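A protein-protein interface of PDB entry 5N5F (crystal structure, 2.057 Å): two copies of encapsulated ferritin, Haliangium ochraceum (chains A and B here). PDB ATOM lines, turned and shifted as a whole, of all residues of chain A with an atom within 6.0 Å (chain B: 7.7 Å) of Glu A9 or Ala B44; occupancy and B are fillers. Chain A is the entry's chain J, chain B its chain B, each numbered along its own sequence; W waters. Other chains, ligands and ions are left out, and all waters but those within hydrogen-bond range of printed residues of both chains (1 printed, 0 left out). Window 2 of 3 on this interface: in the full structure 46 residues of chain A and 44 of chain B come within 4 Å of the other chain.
Water W1 bridges O of Asp B43 (2.8 Å) and O of Leu A13 (3.1 Å).
Glu A9 touches just these residues of chain B: Gln B40 (3.6 Å), Arg B41 (3.8 Å) and Ala B44 (3.5 Å).
Ala B44 touches just these residues of chain A: Glu A9 and Leu A13.
Of the printed residues of chain A, Arg B41 touches Glu A9.
Of the printed residues of chain A, Gln B40 touches Leu A7 (3.6 Å), His A8 (2.7 Å), Glu A9 (3.6 Å) and Leu A14 (3.4 Å).
Of the printed residues of chain B, His A8 touches Trp B37 and Gln B40.
Printed residues of chain B within 4 Å of Leu A14: Gln B40 (3.4 Å) and Asp B43 (3.8 Å).
Ala A11 touches none of the printed residues of chain B.
Glu A12 touches none of the printed residues of chain B.
The nearest residue of chain B that does not touch Glu A9 is Cys B45 (5.7 Å).
Among the printed residues, pairs that only touch across the chains: Leu A14 with Gln B40 (3.4 Å), Glu A9 with Ala B44 (3.5 Å), Leu A7 with Gln B40 (3.6 Å), Glu A9 with Gln B40 (3.6 Å), Leu A13 with Asp B43 (3.7 Å), Leu A14 with Asp B43 (3.8 Å), Glu A9 with Arg B41 (3.8 Å) and Leu A13 with Ala B44 (3.8 Å).
Of the 13 printed residues of chain B, 5 touch a printed residue of chain A.
Hydrophobic or aromatic side chains of chain B that line the printed part of chain A: Trp B37 and Ala B44.
Hydrophobic or aromatic side chains of chain A that line the printed part of chain B: Leu A7, His A8, Leu A13 and Leu A14.
Among the printed residues, 10 pairs touch across the chains.
No position is printed for both chains.
NE2 of Gln B39 is in hydrogen-bond range of OD1 of Asp B43 (2.8 Å).
OE1 of Gln B40 lies within hydrogen-bond range of N of His A8 (2.7 Å).
NE1 of Trp B37 lies close to NE2 of His A8, 3.2 Å away.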
ATOM      1  N   LEU A   7     -13.433 -28.525  14.563  1.00  0.00           N
ATOM      2  CA  LEU A   7     -14.850 -28.205  14.468  1.00  0.00           C
ATOM      3  C   LEU A   7     -15.342 -27.603  15.778  1.00  0.00           C
ATOM      4  O   LEU A   7     -14.960 -28.045  16.864  1.00  0.00           O
ATOM      5  CB  LEU A   7     -15.655 -29.463  14.138  1.00  0.00           C
ATOM      6  CG  LEU A   7     -15.277 -30.183  12.843  1.00  0.00           C
ATOM      7  CD1 LEU A   7     -15.784 -31.615  12.867  1.00  0.00           C
ATOM      8  CD2 LEU A   7     -15.837 -29.437  11.642  1.00  0.00           C
ATOM      9  N   HIS A   8     -16.192 -26.584  15.674  1.00  0.00           N
ATOM     10  CA  HIS A   8     -16.796 -25.961  16.844  1.00  0.00           C
ATOM     11  C   HIS A   8     -18.056 -26.676  17.315  1.00  0.00           C
ATOM     12  O   HIS A   8     -18.607 -26.303  18.355  1.00  0.00           O
ATOM     13  CB  HIS A   8     -17.124 -24.494  16.553  1.00  0.00           C
ATOM     14  CG  HIS A   8     -15.920 -23.606  16.498  1.00  0.00           C
ATOM     15  ND1 HIS A   8     -14.632 -24.092  16.567  1.00  0.00           N
ATOM     16  CD2 HIS A   8     -15.809 -22.261  16.384  1.00  0.00           C
ATOM     17  CE1 HIS A   8     -13.779 -23.086  16.496  1.00  0.00           C
ATOM     18  NE2 HIS A   8     -14.468 -21.964  16.384  1.00  0.00           N
ATOM     19  N   GLU A   9     -18.519 -27.677  16.581  1.00  0.00           N
ATOM     20  CA  GLU A   9     -19.671 -28.482  16.949  1.00  0.00           C
ATOM     21  C   GLU A   9     -19.328 -29.938  16.686  1.00  0.00           C
ATOM     22  O   GLU A   9     -18.467 -30.237  15.851  1.00  0.00           O
ATOM     23  CB  GLU A   9     -20.920 -28.088  16.148  1.00  0.00           C
ATOM     24  CG  GLU A   9     -21.342 -26.630  16.286  1.00  0.00           C
ATOM     25  CD  GLU A   9     -22.155 -26.363  17.545  1.00  0.00           C
ATOM     26  OE1 GLU A   9     -22.449 -27.324  18.289  1.00  0.00           O
ATOM     27  OE2 GLU A   9     -22.509 -25.188  17.785  1.00  0.00           O
ATOM     28  N   PRO A  10     -19.981 -30.871  17.379  1.00  0.00           N
ATOM     29  CA  PRO A  10     -19.716 -32.289  17.113  1.00  0.00           C
ATOM     30  C   PRO A  10     -20.170 -32.678  15.715  1.00  0.00           C
ATOM     31  O   PRO A  10     -21.232 -32.263  15.246  1.00  0.00           O
ATOM     32  CB  PRO A  10     -20.525 -33.015  18.195  1.00  0.00           C
ATOM     33  CG  PRO A  10     -21.600 -32.064  18.562  1.00  0.00           C
ATOM     34  CD  PRO A  10     -21.010 -30.689  18.418  1.00  0.00           C
ATOM     35  N   ALA A  11     -19.346 -33.496  15.053  1.00  0.00           N
ATOM     36  CA  ALA A  11     -19.569 -33.812  13.645  1.00  0.00           C
ATOM     37  C   ALA A  11     -20.959 -34.387  13.399  1.00  0.00           C
ATOM     38  O   ALA A  11     -21.486 -34.274  12.286  1.00  0.00           O
ATOM     39  CB  ALA A  11     -18.501 -34.792  13.158  1.00  0.00           C
ATOM     40  N   GLU A  12     -21.569 -35.000  14.416  1.00  0.00           N
ATOM     41  CA  GLU A  12     -22.876 -35.621  14.226  1.00  0.00           C
ATOM     42  C   GLU A  12     -23.951 -34.588  13.919  1.00  0.00           C
ATOM     43  O   GLU A  12     -24.933 -34.906  13.238  1.00  0.00           O
ATOM     44  CB  GLU A  12     -23.273 -36.425  15.466  1.00  0.00           C
ATOM     45  CG  GLU A  12     -22.180 -37.324  16.026  1.00  0.00           C
ATOM     46  CD  GLU A  12     -21.355 -36.640  17.102  1.00  0.00           C
ATOM     47  OE1 GLU A  12     -20.192 -36.281  16.826  1.00  0.00           O
ATOM     48  OE2 GLU A  12     -21.877 -36.452  18.222  1.00  0.00           O
ATOM     49  N   LEU A  13     -23.793 -33.361  14.409  1.00  0.00           N
ATOM     50  CA  LEU A  13     -24.780 -32.307  14.213  1.00  0.00           C
ATOM     51  C   LEU A  13     -24.538 -31.486  12.950  1.00  0.00           C
ATOM     52  O   LEU A  13     -25.259 -30.508  12.718  1.00  0.00           O
ATOM     53  CB  LEU A  13     -24.798 -31.372  15.428  1.00  0.00           C
ATOM     54  CG  LEU A  13     -25.272 -31.966  16.759  1.00  0.00           C
ATOM     55  CD1 LEU A  13     -25.017 -30.991  17.901  1.00  0.00           C
ATOM     56  CD2 LEU A  13     -26.751 -32.330  16.699  1.00  0.00           C
ATOM     57  N   LEU A  14     -23.555 -31.854  12.132  1.00  0.00           N
ATOM     58  CA  LEU A  14     -23.181 -31.085  10.953  1.00  0.00           C
ATOM     59  C   LEU A  14     -23.490 -31.872   9.685  1.00  0.00           C
ATOM     60  O   LEU A  14     -23.289 -33.089   9.634  1.00  0.00           O
ATOM     61  CB  LEU A  14     -21.693 -30.724  10.987  1.00  0.00           C
ATOM     62  CG  LEU A  14     -21.212 -29.962  12.224  1.00  0.00           C
ATOM     63  CD1 LEU A  14     -19.715 -29.709  12.148  1.00  0.00           C
ATOM     64  CD2 LEU A  14     -21.967 -28.649  12.382  1.00  0.00           C
ATOM     65  N   TRP B  37     -17.552 -20.765  10.985  1.00  0.00           N
ATOM     66  CA  TRP B  37     -18.126 -20.958  12.312  1.00  0.00           C
ATOM     67  C   TRP B  37     -19.628 -20.697  12.330  1.00  0.00           C
ATOM     68  O   TRP B  37     -20.362 -21.364  13.071  1.00  0.00           O
ATOM     69  CB  TRP B  37     -17.417 -20.053  13.318  1.00  0.00           C
ATOM     70  CG  TRP B  37     -15.952 -20.337  13.434  1.00  0.00           C
ATOM     71  CD1 TRP B  37     -15.299 -21.465  13.023  1.00  0.00           C
ATOM     72  CD2 TRP B  37     -14.953 -19.474  13.989  1.00  0.00           C
ATOM     73  NE1 TRP B  37     -13.955 -21.358  13.292  1.00  0.00           N
ATOM     74  CE2 TRP B  37     -13.717 -20.146  13.886  1.00  0.00           C
ATOM     75  CE3 TRP B  37     -14.982 -18.200  14.562  1.00  0.00           C
ATOM     76  CZ2 TRP B  37     -12.524 -19.586  14.336  1.00  0.00           C
ATOM     77  CZ3 TRP B  37     -13.797 -17.646  15.008  1.00  0.00           C
ATOM     78  CH2 TRP B  37     -12.584 -18.338  14.893  1.00  0.00           C
ATOM     79  N   TYR B  38     -20.109 -19.746  11.530  1.00  0.00           N
ATOM     80  CA  TYR B  38     -21.544 -19.481  11.501  1.00  0.00           C
ATOM     81  C   TYR B  38     -22.306 -20.657  10.906  1.00  0.00           C
ATOM     82  O   TYR B  38     -23.358 -21.046  11.423  1.00  0.00           O
ATOM     83  CB  TYR B  38     -21.836 -18.206  10.713  1.00  0.00           C
ATOM     84  CG  TYR B  38     -21.509 -16.923  11.449  1.00  0.00           C
ATOM     85  CD1 TYR B  38     -20.699 -16.922  12.581  1.00  0.00           C
ATOM     86  CD2 TYR B  38     -22.021 -15.710  11.014  1.00  0.00           C
ATOM     87  CE1 TYR B  38     -20.403 -15.745  13.247  1.00  0.00           C
ATOM     88  CE2 TYR B  38     -21.737 -14.531  11.676  1.00  0.00           C
ATOM     89  CZ  TYR B  38     -20.928 -14.552  12.788  1.00  0.00           C
ATOM     90  OH  TYR B  38     -20.646 -13.373  13.438  1.00  0.00           O
ATOM     91  N   GLN B  39     -21.789 -21.241   9.824  1.00  0.00           N
ATOM     92  CA  GLN B  39     -22.463 -22.384   9.222  1.00  0.00           C
ATOM     93  C   GLN B  39     -22.524 -23.554  10.193  1.00  0.00           C
ATOM     94  O   GLN B  39     -23.569 -24.199  10.335  1.00  0.00           O
ATOM     95  CB  GLN B  39     -21.754 -22.791   7.928  1.00  0.00           C
ATOM     96  CG  GLN B  39     -22.481 -23.871   7.143  1.00  0.00           C
ATOM     97  CD  GLN B  39     -23.887 -23.460   6.746  1.00  0.00           C
ATOM     98  OE1 GLN B  39     -24.084 -22.467   6.045  1.00  0.00           O
ATOM     99  NE2 GLN B  39     -24.875 -24.219   7.203  1.00  0.00           N
ATOM    100  N   GLN B  40     -21.416 -23.839  10.880  1.00  0.00           N
ATOM    101  CA  GLN B  40     -21.407 -24.917  11.864  1.00  0.00           C
ATOM    102  C   GLN B  40     -22.446 -24.677  12.956  1.00  0.00           C
ATOM    103  O   GLN B  40     -23.197 -25.586  13.328  1.00  0.00           O
ATOM    104  CB  GLN B  40     -20.015 -25.050  12.477  1.00  0.00           C
ATOM    105  CG  GLN B  40     -18.965 -25.606  11.538  1.00  0.00           C
ATOM    106  CD  GLN B  40     -17.618 -25.752  12.211  1.00  0.00           C
ATOM    107  OE1 GLN B  40     -17.534 -26.138  13.377  1.00  0.00           O
ATOM    108  NE2 GLN B  40     -16.552 -25.435  11.481  1.00  0.00           N
ATOM    109  N   ARG B  41     -22.494 -23.457  13.493  1.00  0.00           N
ATOM    110  CA  ARG B  41     -23.422 -23.175  14.582  1.00  0.00           C
ATOM    111  C   ARG B  41     -24.866 -23.166  14.099  1.00  0.00           C
ATOM    112  O   ARG B  41     -25.765 -23.587  14.838  1.00  0.00           O
ATOM    113  CB  ARG B  41     -23.060 -21.846  15.246  1.00  0.00           C
ATOM    114  CG  ARG B  41     -21.749 -21.910  16.025  1.00  0.00           C
ATOM    115  CD  ARG B  41     -21.657 -20.824  17.084  1.00  0.00           C
ATOM    116  NE  ARG B  41     -21.291 -19.529  16.520  1.00  0.00           N
ATOM    117  CZ  ARG B  41     -20.048 -19.063  16.432  1.00  0.00           C
ATOM    118  NH1 ARG B  41     -19.022 -19.779  16.873  1.00  0.00           N
ATOM    119  NH2 ARG B  41     -19.832 -17.867  15.900  1.00  0.00           N
ATOM    120  N   ALA B  42     -25.111 -22.714  12.866  1.00  0.00           N
ATOM    121  CA  ALA B  42     -26.464 -22.755  12.321  1.00  0.00           C
ATOM    122  C   ALA B  42     -26.920 -24.191  12.084  1.00  0.00           C
ATOM    123  O   ALA B  42     -28.101 -24.511  12.271  1.00  0.00           O
ATOM    124  CB  ALA B  42     -26.535 -21.949  11.027  1.00  0.00           C
ATOM    125  N   ASP B  43     -26.000 -25.070  11.682  1.00  0.00           N
ATOM    126  CA  ASP B  43     -26.344 -26.476  11.491  1.00  0.00           C
ATOM    127  C   ASP B  43     -26.782 -27.122  12.799  1.00  0.00           C
ATOM    128  O   ASP B  43     -27.813 -27.801  12.857  1.00  0.00           O
ATOM    129  CB  ASP B  43     -25.152 -27.231  10.905  1.00  0.00           C
ATOM    130  CG  ASP B  43     -25.123 -27.196   9.393  1.00  0.00           C
ATOM    131  OD1 ASP B  43     -25.774 -26.301   8.808  1.00  0.00           O
ATOM    132  OD2 ASP B  43     -24.447 -28.061   8.792  1.00  0.00           O
ATOM    133  N   ALA B  44     -25.989 -26.945  13.856  1.00  0.00           N
ATOM    134  CA  ALA B  44     -26.310 -27.525  15.151  1.00  0.00           C
ATOM    135  C   ALA B  44     -27.416 -26.769  15.872  1.00  0.00           C
ATOM    136  O   ALA B  44     -27.979 -27.298  16.836  1.00  0.00           O
ATOM    137  CB  ALA B  44     -25.058 -27.567  16.028  1.00  0.00           C
ATOM    138  N   CYS B  45     -27.734 -25.555  15.427  1.00  0.00           N
ATOM    139  CA  CYS B  45     -28.815 -24.778  16.015  1.00  0.00           C
ATOM    140  C   CYS B  45     -30.098 -25.597  16.061  1.00  0.00           C
ATOM    141  O   CYS B  45     -30.383 -26.383  15.154  1.00  0.00           O
ATOM    142  CB  CYS B  45     -29.036 -23.505  15.196  1.00  0.00           C
ATOM    143  SG  CYS B  45     -29.662 -22.093  16.123  1.00  0.00           S
ATOM    144  N   SER B  46     -30.871 -25.410  17.132  1.00  0.00           N
ATOM    145  CA  SER B  46     -32.169 -26.053  17.283  1.00  0.00           C
ATOM    146  C   SER B  46     -33.318 -25.057  17.350  1.00  0.00           C
ATOM    147  O   SER B  46     -34.465 -25.469  17.557  1.00  0.00           O
ATOM    148  CB  SER B  46     -32.187 -26.935  18.539  1.00  0.00           C
ATOM    149  OG  SER B  46     -31.787 -26.197  19.682  1.00  0.00           O
ATOM    150  N   GLU B  47     -33.049 -23.765  17.184  1.00  0.00           N
ATOM    151  CA  GLU B  47     -34.072 -22.729  17.221  1.00  0.00           C
ATOM    152  C   GLU B  47     -34.118 -22.044  15.860  1.00  0.00           C
ATOM    153  O   GLU B  47     -33.086 -21.516  15.409  1.00  0.00           O
ATOM    154  CB  GLU B  47     -33.768 -21.717  18.328  1.00  0.00           C
ATOM    155  CG  GLU B  47     -34.995 -21.011  18.882  1.00  0.00           C
ATOM    156  CD  GLU B  47     -35.495 -19.906  17.975  1.00  0.00           C
ATOM    157  OE1 GLU B  47     -34.662 -19.118  17.484  1.00  0.00           O
ATOM    158  OE2 GLU B  47     -36.721 -19.829  17.747  1.00  0.00           O
ATOM    159  N   HIS B  51     -31.134 -19.625  13.893  1.00  0.00           N
ATOM    160  CA  HIS B  51     -30.583 -20.129  12.640  1.00  0.00           C
ATOM    161  C   HIS B  51     -30.587 -19.050  11.565  1.00  0.00           C
ATOM    162  O   HIS B  51     -29.560 -18.782  10.933  1.00  0.00           O
ATOM    163  CB  HIS B  51     -31.381 -21.351  12.180  1.00  0.00           C
ATOM    164  CG  HIS B  51     -30.983 -21.861  10.829  1.00  0.00           C
ATOM    165  ND1 HIS B  51     -31.506 -21.356   9.659  1.00  0.00           N
ATOM    166  CD2 HIS B  51     -30.118 -22.837  10.465  1.00  0.00           C
ATOM    167  CE1 HIS B  51     -30.976 -21.996   8.630  1.00  0.00           C
ATOM    168  NE2 HIS B  51     -30.132 -22.900   9.092  1.00  0.00           N
ATOM    169  N   LEU B  54     -28.057 -16.353  12.053  1.00  0.00           N
ATOM    170  CA  LEU B  54     -26.692 -16.805  11.812  1.00  0.00           C
ATOM    171  C   LEU B  54     -26.384 -16.863  10.320  1.00  0.00           C
ATOM    172  O   LEU B  54     -25.304 -16.446   9.887  1.00  0.00           O
ATOM    173  CB  LEU B  54     -26.476 -18.173  12.458  1.00  0.00           C
ATOM    174  CG  LEU B  54     -26.333 -18.207  13.982  1.00  0.00           C
ATOM    175  CD1 LEU B  54     -26.316 -19.643  14.469  1.00  0.00           C
ATOM    176  CD2 LEU B  54     -25.077 -17.478  14.444  1.00  0.00           C
HETATM  177  O   HOH W   1     -28.223 -30.527  13.467  1.00  0.00           O
